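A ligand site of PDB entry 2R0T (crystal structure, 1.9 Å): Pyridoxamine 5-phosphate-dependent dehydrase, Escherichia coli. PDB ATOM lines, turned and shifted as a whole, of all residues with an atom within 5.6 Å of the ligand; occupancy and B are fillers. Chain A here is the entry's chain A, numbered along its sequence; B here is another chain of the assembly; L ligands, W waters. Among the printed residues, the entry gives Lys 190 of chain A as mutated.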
ATOM      1  N   SER A  57      28.141 -20.812  -8.354  1.00  0.00           N
ATOM      2  CA  SER A  57      27.690 -19.495  -7.982  1.00  0.00           C
ATOM      3  C   SER A  57      28.900 -18.770  -7.492  1.00  0.00           C
ATOM      4  O   SER A  57      29.929 -19.384  -7.304  1.00  0.00           O
ATOM      5  CB  SER A  57      26.670 -19.576  -6.852  1.00  0.00           C
ATOM      6  OG  SER A  57      27.207 -20.106  -5.613  1.00  0.00           O
ATOM      7  N   GLY A  58      28.804 -17.450  -7.297  1.00  0.00           N
ATOM      8  CA  GLY A  58      29.964 -16.763  -6.737  1.00  0.00           C
ATOM      9  C   GLY A  58      30.276 -17.193  -5.282  1.00  0.00           C
ATOM     10  O   GLY A  58      31.413 -17.097  -4.815  1.00  0.00           O
ATOM     11  N   SER A  59      29.291 -17.708  -4.565  1.00  0.00           N
ATOM     12  CA  SER A  59      29.500 -18.116  -3.169  1.00  0.00           C
ATOM     13  C   SER A  59      30.429 -19.340  -3.176  1.00  0.00           C
ATOM     14  O   SER A  59      31.436 -19.422  -2.452  1.00  0.00           O
ATOM     15  CB  SER A  59      28.104 -18.416  -2.567  1.00  0.00           C
ATOM     16  OG  SER A  59      27.470 -17.191  -2.253  1.00  0.00           O
ATOM     17  N   THR A  60      30.095 -20.306  -4.014  1.00  0.00           N
ATOM     18  CA  THR A  60      30.937 -21.480  -4.069  1.00  0.00           C
ATOM     19  C   THR A  60      32.278 -21.166  -4.703  1.00  0.00           C
ATOM     20  O   THR A  60      33.213 -21.943  -4.515  1.00  0.00           O
ATOM     21  CB  THR A  60      30.272 -22.633  -4.793  1.00  0.00           C
ATOM     22  OG1 THR A  60      29.975 -22.257  -6.139  1.00  0.00           O
ATOM     23  CG2 THR A  60      29.025 -23.042  -4.044  1.00  0.00           C
ATOM     24  N   ASN A  62      33.883 -18.461  -3.872  1.00  0.00           N
ATOM     25  CA  ASN A  62      34.607 -18.084  -2.678  1.00  0.00           C
ATOM     26  C   ASN A  62      34.995 -19.313  -1.849  1.00  0.00           C
ATOM     27  O   ASN A  62      36.065 -19.365  -1.221  1.00  0.00           O
ATOM     28  CB  ASN A  62      33.741 -17.140  -1.827  1.00  0.00           C
ATOM     29  CG  ASN A  62      33.677 -15.739  -2.417  1.00  0.00           C
ATOM     30  OD1 ASN A  62      34.374 -15.460  -3.379  1.00  0.00           O
ATOM     31  ND2 ASN A  62      32.862 -14.864  -1.843  1.00  0.00           N
ATOM     32  N   SER A  89      30.728  -6.384   3.055  1.00  0.00           N
ATOM     33  CA  SER A  89      30.722  -7.304   1.906  1.00  0.00           C
ATOM     34  C   SER A  89      29.516  -8.196   2.099  1.00  0.00           C
ATOM     35  O   SER A  89      28.865  -8.117   3.142  1.00  0.00           O
ATOM     36  CB  SER A  89      31.992  -8.176   1.930  1.00  0.00           C
ATOM     37  OG  SER A  89      32.129  -8.833   0.687  1.00  0.00           O
ATOM     38  N   TRP A  90      29.293  -9.080   1.122  1.00  0.00           N
ATOM     39  CA  TRP A  90      28.291 -10.146   1.208  1.00  0.00           C
ATOM     40  C   TRP A  90      28.709 -11.223   2.243  1.00  0.00           C
ATOM     41  O   TRP A  90      29.912 -11.511   2.552  1.00  0.00           O
ATOM     42  CB  TRP A  90      28.122 -10.812  -0.159  1.00  0.00           C
ATOM     43  CG  TRP A  90      26.924 -11.696  -0.188  1.00  0.00           C
ATOM     44  CD1 TRP A  90      26.878 -13.051  -0.370  1.00  0.00           C
ATOM     45  CD2 TRP A  90      25.589 -11.280   0.048  1.00  0.00           C
ATOM     46  NE1 TRP A  90      25.562 -13.500  -0.297  1.00  0.00           N
ATOM     47  CE2 TRP A  90      24.770 -12.419  -0.042  1.00  0.00           C
ATOM     48  CE3 TRP A  90      25.011 -10.036   0.279  1.00  0.00           C
ATOM     49  CZ2 TRP A  90      23.411 -12.354   0.166  1.00  0.00           C
ATOM     50  CZ3 TRP A  90      23.654  -9.947   0.398  1.00  0.00           C
ATOM     51  CH2 TRP A  90      22.865 -11.111   0.366  1.00  0.00           C
ATOM     52  N   THR A  92      28.762 -14.406   2.165  1.00  0.00           N
ATOM     53  CA  THR A  92      29.501 -15.589   1.758  1.00  0.00           C
ATOM     54  C   THR A  92      30.902 -15.224   1.417  1.00  0.00           C
ATOM     55  O   THR A  92      31.621 -16.047   0.929  1.00  0.00           O
ATOM     56  CB  THR A  92      28.894 -16.401   0.626  1.00  0.00           C
ATOM     57  OG1 THR A  92      28.806 -15.576  -0.544  1.00  0.00           O
ATOM     58  CG2 THR A  92      27.540 -16.987   0.975  1.00  0.00           C
ATOM     59  N   THR A  93      31.317 -13.992   1.649  1.00  0.00           N
ATOM     60  CA  THR A  93      32.737 -13.677   1.499  1.00  0.00           C
ATOM     61  C   THR A  93      33.348 -14.210   2.810  1.00  0.00           C
ATOM     62  O   THR A  93      34.484 -14.656   2.873  1.00  0.00           O
ATOM     63  CB  THR A  93      32.923 -12.170   1.626  1.00  0.00           C
ATOM     64  OG1 THR A  93      32.304 -11.548   0.502  1.00  0.00           O
ATOM     65  CG2 THR A  93      34.369 -11.806   1.693  1.00  0.00           C
ATOM     66  N   VAL A 135      37.760  -7.074  -1.311  1.00  0.00           N
ATOM     67  CA  VAL A 135      36.504  -7.168  -2.037  1.00  0.00           C
ATOM     68  C   VAL A 135      36.453  -5.884  -2.860  1.00  0.00           C
ATOM     69  O   VAL A 135      36.689  -4.845  -2.272  1.00  0.00           O
ATOM     70  CB  VAL A 135      35.354  -7.179  -1.007  1.00  0.00           C
ATOM     71  CG1 VAL A 135      33.988  -7.105  -1.683  1.00  0.00           C
ATOM     72  CG2 VAL A 135      35.416  -8.429  -0.121  1.00  0.00           C
ATOM     73  N   ASP A 161      37.570 -10.954  -3.765  1.00  0.00           N
ATOM     74  CA  ASP A 161      36.158 -11.276  -4.064  1.00  0.00           C
ATOM     75  C   ASP A 161      35.749 -10.124  -5.052  1.00  0.00           C
ATOM     76  O   ASP A 161      35.671  -8.925  -4.711  1.00  0.00           O
ATOM     77  CB  ASP A 161      35.266 -11.304  -2.843  1.00  0.00           C
ATOM     78  CG  ASP A 161      33.800 -11.519  -3.196  1.00  0.00           C
ATOM     79  OD1 ASP A 161      33.368 -11.411  -4.361  1.00  0.00           O
ATOM     80  OD2 ASP A 161      33.053 -11.759  -2.250  1.00  0.00           O
ATOM     81  N   CYS A 163      32.986 -10.271  -6.911  1.00  0.00           N
ATOM     82  CA  CYS A 163      31.635 -10.613  -7.361  1.00  0.00           C
ATOM     83  C   CYS A 163      30.741  -9.471  -7.799  1.00  0.00           C
ATOM     84  O   CYS A 163      29.702  -9.661  -8.442  1.00  0.00           O
ATOM     85  CB  CYS A 163      30.957 -11.492  -6.315  1.00  0.00           C
ATOM     86  SG  CYS A 163      31.738 -13.140  -6.349  1.00  0.00           S
ATOM     87  N   GLU A 164      31.121  -8.267  -7.375  1.00  0.00           N
ATOM     88  CA  GLU A 164      30.393  -7.008  -7.703  1.00  0.00           C
ATOM     89  C   GLU A 164      31.085  -6.077  -8.701  1.00  0.00           C
ATOM     90  O   GLU A 164      30.563  -5.012  -9.023  1.00  0.00           O
ATOM     91  CB  GLU A 164      30.114  -6.186  -6.425  1.00  0.00           C
ATOM     92  CG  GLU A 164      29.383  -6.981  -5.366  1.00  0.00           C
ATOM     93  CD  GLU A 164      29.019  -6.193  -4.106  1.00  0.00           C
ATOM     94  OE1 GLU A 164      29.482  -5.036  -3.952  1.00  0.00           O
ATOM     95  OE2 GLU A 164      28.264  -6.733  -3.267  1.00  0.00           O
ATOM     96  N   SER A 185      30.870 -13.515 -10.119  1.00  0.00           N
ATOM     97  CA  SER A 185      29.518 -14.073  -9.977  1.00  0.00           C
ATOM     98  C   SER A 185      28.729 -13.757 -11.193  1.00  0.00           C
ATOM     99  O   SER A 185      28.783 -12.614 -11.633  1.00  0.00           O
ATOM    100  CB  SER A 185      28.823 -13.372  -8.815  1.00  0.00           C
ATOM    101  OG  SER A 185      27.480 -13.772  -8.724  1.00  0.00           O
ATOM    102  N   SER A 186      27.996 -14.728 -11.758  1.00  0.00           N
ATOM    103  CA  SER A 186      27.059 -14.396 -12.876  1.00  0.00           C
ATOM    104  C   SER A 186      25.574 -14.625 -12.495  1.00  0.00           C
ATOM    105  O   SER A 186      24.723 -14.980 -13.315  1.00  0.00           O
ATOM    106  CB  SER A 186      27.390 -15.089 -14.186  1.00  0.00           C
ATOM    107  OG  SER A 186      27.765 -16.399 -13.862  1.00  0.00           O
ATOM    108  N   PHE A 187      25.304 -14.382 -11.217  1.00  0.00           N
ATOM    109  CA  PHE A 187      23.975 -14.416 -10.654  1.00  0.00           C
ATOM    110  C   PHE A 187      23.140 -13.325 -11.350  1.00  0.00           C
ATOM    111  O   PHE A 187      23.660 -12.282 -11.794  1.00  0.00           O
ATOM    112  CB  PHE A 187      24.026 -14.147  -9.156  1.00  0.00           C
ATOM    113  CG  PHE A 187      22.670 -14.122  -8.499  1.00  0.00           C
ATOM    114  CD1 PHE A 187      21.926 -15.297  -8.364  1.00  0.00           C
ATOM    115  CD2 PHE A 187      22.127 -12.940  -8.006  1.00  0.00           C
ATOM    116  CE1 PHE A 187      20.680 -15.284  -7.765  1.00  0.00           C
ATOM    117  CE2 PHE A 187      20.885 -12.918  -7.397  1.00  0.00           C
ATOM    118  CZ  PHE A 187      20.170 -14.100  -7.257  1.00  0.00           C
ATOM    119  N   SER A 189      21.334 -10.775 -10.797  1.00  0.00           N
ATOM    120  CA  SER A 189      21.511  -9.332 -10.535  1.00  0.00           C
ATOM    121  C   SER A 189      22.854  -8.688 -10.805  1.00  0.00           C
ATOM    122  O   SER A 189      22.978  -7.444 -10.721  1.00  0.00           O
ATOM    123  CB  SER A 189      21.142  -9.076  -9.087  1.00  0.00           C
ATOM    124  OG  SER A 189      22.045  -9.764  -8.221  1.00  0.00           O
ATOM    125  N   LYS A 190      23.866  -9.480 -11.183  1.00  0.00           N
ATOM    126  CA  LYS A 190      25.240  -9.059 -11.476  1.00  0.00           C
ATOM    127  C   LYS A 190      25.548  -8.417 -12.900  1.00  0.00           C
ATOM    128  O   LYS A 190      24.626  -7.951 -13.579  1.00  0.00           O
ATOM    129  CB  LYS A 190      26.253 -10.016 -10.776  1.00  0.00           C
ATOM    130  CG  LYS A 190      25.767 -10.161  -9.348  1.00  0.00           C
ATOM    131  CD  LYS A 190      26.762 -10.509  -8.265  1.00  0.00           C
ATOM    132  CE  LYS A 190      26.092 -11.024  -6.995  1.00  0.00           C
ATOM    133  NZ  LYS A 190      26.691 -10.375  -5.796  1.00  0.00           N
ATOM    134  N   GLU A 196      22.468 -18.698 -12.407  1.00  0.00           N
ATOM    135  CA  GLU A 196      23.365 -18.702 -11.238  1.00  0.00           C
ATOM    136  C   GLU A 196      24.716 -19.034 -11.871  1.00  0.00           C
ATOM    137  O   GLU A 196      24.760 -19.615 -12.953  1.00  0.00           O
ATOM    138  CB  GLU A 196      23.047 -19.751 -10.166  1.00  0.00           C
ATOM    139  CG  GLU A 196      21.788 -19.529  -9.356  1.00  0.00           C
ATOM    140  CD  GLU A 196      21.975 -19.099  -7.918  1.00  0.00           C
ATOM    141  OE1 GLU A 196      23.003 -18.491  -7.524  1.00  0.00           O
ATOM    142  OE2 GLU A 196      20.969 -19.326  -7.209  1.00  0.00           O
ATOM    143  N   GLY A 197      25.821 -18.695 -11.225  1.00  0.00           N
ATOM    144  CA  GLY A 197      27.133 -19.075 -11.754  1.00  0.00           C
ATOM    145  C   GLY A 197      28.183 -18.222 -11.085  1.00  0.00           C
ATOM    146  O   GLY A 197      27.921 -17.121 -10.624  1.00  0.00           O
ATOM    147  N   GLY A 198      29.392 -18.753 -11.014  1.00  0.00           N
ATOM    148  CA  GLY A 198      30.528 -18.000 -10.454  1.00  0.00           C
ATOM    149  C   GLY A 198      31.784 -18.509 -11.151  1.00  0.00           C
ATOM    150  O   GLY A 198      31.749 -19.501 -11.891  1.00  0.00           O
ATOM    151  N   PHE A 304      28.591  -1.036 -10.408  1.00  0.00           N
ATOM    152  CA  PHE A 304      27.514  -1.964 -10.162  1.00  0.00           C
ATOM    153  C   PHE A 304      26.212  -1.248  -9.760  1.00  0.00           C
ATOM    154  O   PHE A 304      25.115  -1.599 -10.187  1.00  0.00           O
ATOM    155  CB  PHE A 304      28.028  -2.908  -9.092  1.00  0.00           C
ATOM    156  CG  PHE A 304      27.027  -3.880  -8.594  1.00  0.00           C
ATOM    157  CD1 PHE A 304      26.738  -5.022  -9.335  1.00  0.00           C
ATOM    158  CD2 PHE A 304      26.491  -3.736  -7.329  1.00  0.00           C
ATOM    159  CE1 PHE A 304      25.850  -5.974  -8.848  1.00  0.00           C
ATOM    160  CE2 PHE A 304      25.574  -4.669  -6.827  1.00  0.00           C
ATOM    161  CZ  PHE A 304      25.277  -5.813  -7.584  1.00  0.00           C
ATOM    162  N   ARG A 333      18.198  -0.274  -1.250  1.00  0.00           N
ATOM    163  CA  ARG A 333      18.501  -1.247  -0.215  1.00  0.00           C
ATOM    164  C   ARG A 333      19.727  -0.688   0.518  1.00  0.00           C
ATOM    165  O   ARG A 333      20.259   0.376   0.177  1.00  0.00           O
ATOM    166  CB  ARG A 333      18.853  -2.566  -0.869  1.00  0.00           C
ATOM    167  CG  ARG A 333      19.910  -2.298  -1.931  1.00  0.00           C
ATOM    168  CD  ARG A 333      20.357  -3.553  -2.655  1.00  0.00           C
ATOM    169  NE  ARG A 333      21.358  -4.228  -1.816  1.00  0.00           N
ATOM    170  CZ  ARG A 333      21.902  -5.425  -2.045  1.00  0.00           C
ATOM    171  NH1 ARG A 333      21.504  -6.157  -3.080  1.00  0.00           N
ATOM    172  NH2 ARG A 333      22.816  -5.909  -1.223  1.00  0.00           N
ATOM    173  N   VAL A 336      25.273  -2.981   0.077  1.00  0.00           N
ATOM    174  CA  VAL A 336      25.720  -4.375   0.186  1.00  0.00           C
ATOM    175  C   VAL A 336      24.913  -4.909   1.349  1.00  0.00           C
ATOM    176  O   VAL A 336      23.708  -4.924   1.252  1.00  0.00           O
ATOM    177  CB  VAL A 336      27.247  -4.520   0.440  1.00  0.00           C
ATOM    178  CG1 VAL A 336      27.545  -5.965   0.319  1.00  0.00           C
ATOM    179  CG2 VAL A 336      27.963  -3.749  -0.641  1.00  0.00           C
ATOM    180  N   HIS B 217      22.751 -18.428   1.917  1.00  0.00           N
ATOM    181  CA  HIS B 217      23.475 -17.331   2.561  1.00  0.00           C
ATOM    182  C   HIS B 217      23.356 -17.158   4.067  1.00  0.00           C
ATOM    183  O   HIS B 217      23.948 -16.217   4.632  1.00  0.00           O
ATOM    184  CB  HIS B 217      22.991 -16.048   1.864  1.00  0.00           C
ATOM    185  CG  HIS B 217      23.174 -16.075   0.383  1.00  0.00           C
ATOM    186  ND1 HIS B 217      24.423 -15.974  -0.208  1.00  0.00           N
ATOM    187  CD2 HIS B 217      22.289 -16.240  -0.626  1.00  0.00           C
ATOM    188  CE1 HIS B 217      24.286 -16.066  -1.519  1.00  0.00           C
ATOM    189  NE2 HIS B 217      23.000 -16.207  -1.797  1.00  0.00           N
ATOM    190  N   TRP B 219      20.616 -16.330   5.418  1.00  0.00           N
ATOM    191  CA  TRP B 219      19.711 -15.203   5.682  1.00  0.00           C
ATOM    192  C   TRP B 219      18.372 -15.743   6.210  1.00  0.00           C
ATOM    193  O   TRP B 219      18.226 -16.953   6.383  1.00  0.00           O
ATOM    194  CB  TRP B 219      19.524 -14.268   4.483  1.00  0.00           C
ATOM    195  CG  TRP B 219      18.962 -14.986   3.292  1.00  0.00           C
ATOM    196  CD1 TRP B 219      18.226 -16.159   3.278  1.00  0.00           C
ATOM    197  CD2 TRP B 219      19.046 -14.540   1.933  1.00  0.00           C
ATOM    198  NE1 TRP B 219      17.845 -16.455   1.979  1.00  0.00           N
ATOM    199  CE2 TRP B 219      18.318 -15.467   1.145  1.00  0.00           C
ATOM    200  CE3 TRP B 219      19.653 -13.441   1.313  1.00  0.00           C
ATOM    201  CZ2 TRP B 219      18.233 -15.361  -0.258  1.00  0.00           C
ATOM    202  CZ3 TRP B 219      19.551 -13.314  -0.082  1.00  0.00           C
ATOM    203  CH2 TRP B 219      18.815 -14.255  -0.845  1.00  0.00           C
ATOM    204  N   ARG B 221      15.363 -14.679   4.886  1.00  0.00           N
ATOM    205  CA  ARG B 221      14.423 -14.545   3.813  1.00  0.00           C
ATOM    206  C   ARG B 221      13.537 -15.745   3.548  1.00  0.00           C
ATOM    207  O   ARG B 221      12.411 -15.527   3.184  1.00  0.00           O
ATOM    208  CB  ARG B 221      15.137 -14.104   2.532  1.00  0.00           C
ATOM    209  CG  ARG B 221      15.699 -12.695   2.657  1.00  0.00           C
ATOM    210  CD  ARG B 221      15.950 -12.158   1.266  1.00  0.00           C
ATOM    211  NE  ARG B 221      16.949 -11.117   1.328  1.00  0.00           N
ATOM    212  CZ  ARG B 221      17.550 -10.605   0.259  1.00  0.00           C
ATOM    213  NH1 ARG B 221      17.256 -11.025  -0.965  1.00  0.00           N
ATOM    214  NH2 ARG B 221      18.463  -9.652   0.427  1.00  0.00           N
ATOM    215  N   ASN B 250      25.552 -21.002  -0.584  1.00  0.00           N
ATOM    216  CA  ASN B 250      24.651 -20.733  -1.709  1.00  0.00           C
ATOM    217  C   ASN B 250      24.615 -22.050  -2.439  1.00  0.00           C
ATOM    218  O   ASN B 250      25.568 -22.365  -3.156  1.00  0.00           O
ATOM    219  CB  ASN B 250      25.081 -19.608  -2.683  1.00  0.00           C
ATOM    220  CG  ASN B 250      24.089 -19.493  -3.798  1.00  0.00           C
ATOM    221  OD1 ASN B 250      23.139 -20.271  -3.766  1.00  0.00           O
ATOM    222  ND2 ASN B 250      24.254 -18.580  -4.757  1.00  0.00           N
ATOM    223  N   ARG B 252      21.420 -23.212  -3.726  1.00  0.00           N
ATOM    224  CA  ARG B 252      20.052 -23.087  -4.281  1.00  0.00           C
ATOM    225  C   ARG B 252      19.992 -23.798  -5.590  1.00  0.00           C
ATOM    226  O   ARG B 252      20.918 -23.707  -6.395  1.00  0.00           O
ATOM    227  CB  ARG B 252      19.781 -21.604  -4.616  1.00  0.00           C
ATOM    228  CG  ARG B 252      19.580 -20.803  -3.340  1.00  0.00           C
ATOM    229  CD  ARG B 252      19.246 -19.316  -3.695  1.00  0.00           C
ATOM    230  NE  ARG B 252      20.151 -18.744  -4.683  1.00  0.00           N
ATOM    231  CZ  ARG B 252      20.592 -17.475  -4.685  1.00  0.00           C
ATOM    232  NH1 ARG B 252      20.156 -16.645  -3.745  1.00  0.00           N
ATOM    233  NH2 ARG B 252      21.474 -17.048  -5.608  1.00  0.00           N
HETATM  234  N1  LIG L   1      30.589 -11.982  -3.021  1.00  0.00           N
HETATM  235  C1  LIG L   1      30.178 -10.750  -3.207  1.00  0.00           C
HETATM  236  C2  LIG L   1      31.118  -9.656  -2.783  1.00  0.00           C
HETATM  237  C3  LIG L   1      28.902 -10.488  -3.777  1.00  0.00           C
HETATM  238  O1  LIG L   1      28.441  -9.233  -3.984  1.00  0.00           O
HETATM  239  C4  LIG L   1      28.042 -11.551  -4.102  1.00  0.00           C
HETATM  240  C5  LIG L   1      26.656 -11.285  -4.646  1.00  0.00           C
HETATM  241  C6  LIG L   1      28.510 -12.857  -3.814  1.00  0.00           C
HETATM  242  C7  LIG L   1      29.798 -13.027  -3.319  1.00  0.00           C
HETATM  243  C8  LIG L   1      27.640 -14.058  -4.036  1.00  0.00           C
HETATM  244  O2  LIG L   1      27.731 -14.498  -5.333  1.00  0.00           O
HETATM  245  P1  LIG L   1      26.466 -15.368  -5.669  1.00  0.00           P
HETATM  246  O3  LIG L   1      26.638 -15.794  -7.200  1.00  0.00           O
HETATM  247  O4  LIG L   1      25.161 -14.514  -5.481  1.00  0.00           O
HETATM  248  O5  LIG L   1      26.334 -16.563  -4.663  1.00  0.00           O
HETATM  249  N2  LIG L   1      25.780 -10.758  -3.568  1.00  0.00           N
HETATM  250  C9  LIG L   1      24.338 -10.690  -3.998  1.00  0.00           C
HETATM  251  C10 LIG L   1      23.597 -11.905  -3.415  1.00  0.00           C
HETATM  252  C11 LIG L   1      22.497 -12.310  -4.373  1.00  0.00           C
HETATM  253  C12 LIG L   1      22.163 -13.777  -4.201  1.00  0.00           C
HETATM  254  O6  LIG L   1      21.010 -14.096  -3.766  1.00  0.00           O
HETATM  255  O7  LIG L   1      23.050 -14.703  -4.487  1.00  0.00           O
HETATM  256  C13 LIG L   1      23.696  -9.393  -3.443  1.00  0.00           C
HETATM  257  O8  LIG L   1      22.418  -9.329  -3.311  1.00  0.00           O
HETATM  258  O9  LIG L   1      24.433  -8.400  -3.072  1.00  0.00           O
HETATM  259  O   HOH W   1      25.093 -17.388  -8.667  1.00  0.00           O
HETATM  260  O   HOH W   2      19.267 -11.704  -4.028  1.00  0.00           O
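O1 of the ligand is in hydrogen-bond range of OE2 of Glu 164, at 2.6 Å. The guanidinium group (NH1) of Arg 333 lies within salt-bridge range of an oxygen (O8) of the ligand (3.3 Å). The side-chain amide nitrogen of Asn 250 of chain B sits at hydrogen-bond distance from an oxygen (O5) of the ligand (2.9 Å). N of Ser 59 lies within hydrogen-bond range of O5 of the ligand, 3.2 Å away. The side-chain sulfur of Cys 163 sits close to a nitrogen (N1) of the ligand, at 3.7 Å. An oxygen (O7) of the ligand lies within hydrogen-bond range of a ring nitrogen (NE2) of His 217 of chain B (3.1 Å). The backbone NH (N) of Gly 58 lies within hydrogen-bond range of an oxygen (O3) of the ligand (2.7 Å). OG of Ser 59 sits at hydrogen-bond distance from O5 of the ligand. The guanidinium group (NH1) of Arg 252 of chain B is in salt-bridge range of an oxygen (O6) of the ligand (2.7 Å). The side-chain amino group (NZ) of Lys 190 is covalently linked to a carbon (C5) of the ligand, at 1.5 Å. The side-chain carboxylate of Asp 161 sits at hydrogen-bond distance from a nitrogen (N1) of the ligand (2.6 Å). The side-chain hydroxyl (OG) of Ser 185 sits at hydrogen-bond distance from an oxygen (O3) of the ligand (2.7 Å).
Water W1 lies within hydrogen-bond range of the side-chain carboxylate of Glu 196 (2.6 Å), an oxygen (O3) of the ligand (2.7 Å) and the backbone NH of Gly 197 (3.0 Å).
Residues that only touch the ligand: Phe 187 (3.5 Å), Trp 90 (3.6 Å), Trp 219 of chain B (3.7 Å), Ser 89 (3.7 Å), Ser 57 (3.7 Å), Asn 62 (3.9 Å), Gly 197 (3.9 Å), Thr 92 (3.9 Å), Thr 93 (3.9 Å) and Val 135 (3.99 Å). Hydrophobic or aromatic side chains that line the ligand: Trp 90, Val 135, Phe 187, His 217 of chain B and Trp 219 of chain B. Of the 29 residues printed, 21 come within 4 Å of the ligand.
The side-chain hydroxyl (OG1) of Thr 93 is in hydrogen-bond range of the side-chain hydroxyl (OG) of Ser 89 (2.7 Å). The backbone carbonyl oxygen of Trp 90 lies within hydrogen-bond range of the side-chain hydroxyl of Thr 93. The guanidinium group (NH2) of Arg 252 of chain B lies close to the side-chain amide nitrogen (ND2) of Asn 250 of chain B (3.3 Å). The backbone NH (N) of Ser 186 lies within hydrogen-bond range of the backbone carbonyl oxygen (O) of Gly 197 (2.6 Å). The side-chain carboxylate (OD2) of Asp 161 sits at hydrogen-bond distance from the side-chain hydroxyl (OG1) of Thr 93 (2.9 Å). The side-chain hydroxyl (OG) of Ser 57 sits close to the side-chain amide nitrogen (ND2) of Asn 250 of chain B (3.4 Å). The backbone NH (N) of Ser 59 sits close to the side-chain hydroxyl (OG) of Ser 57 (3.3 Å). O of Gly 197 sits at hydrogen-bond distance from N of Gly 58, 3.5 Å away.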
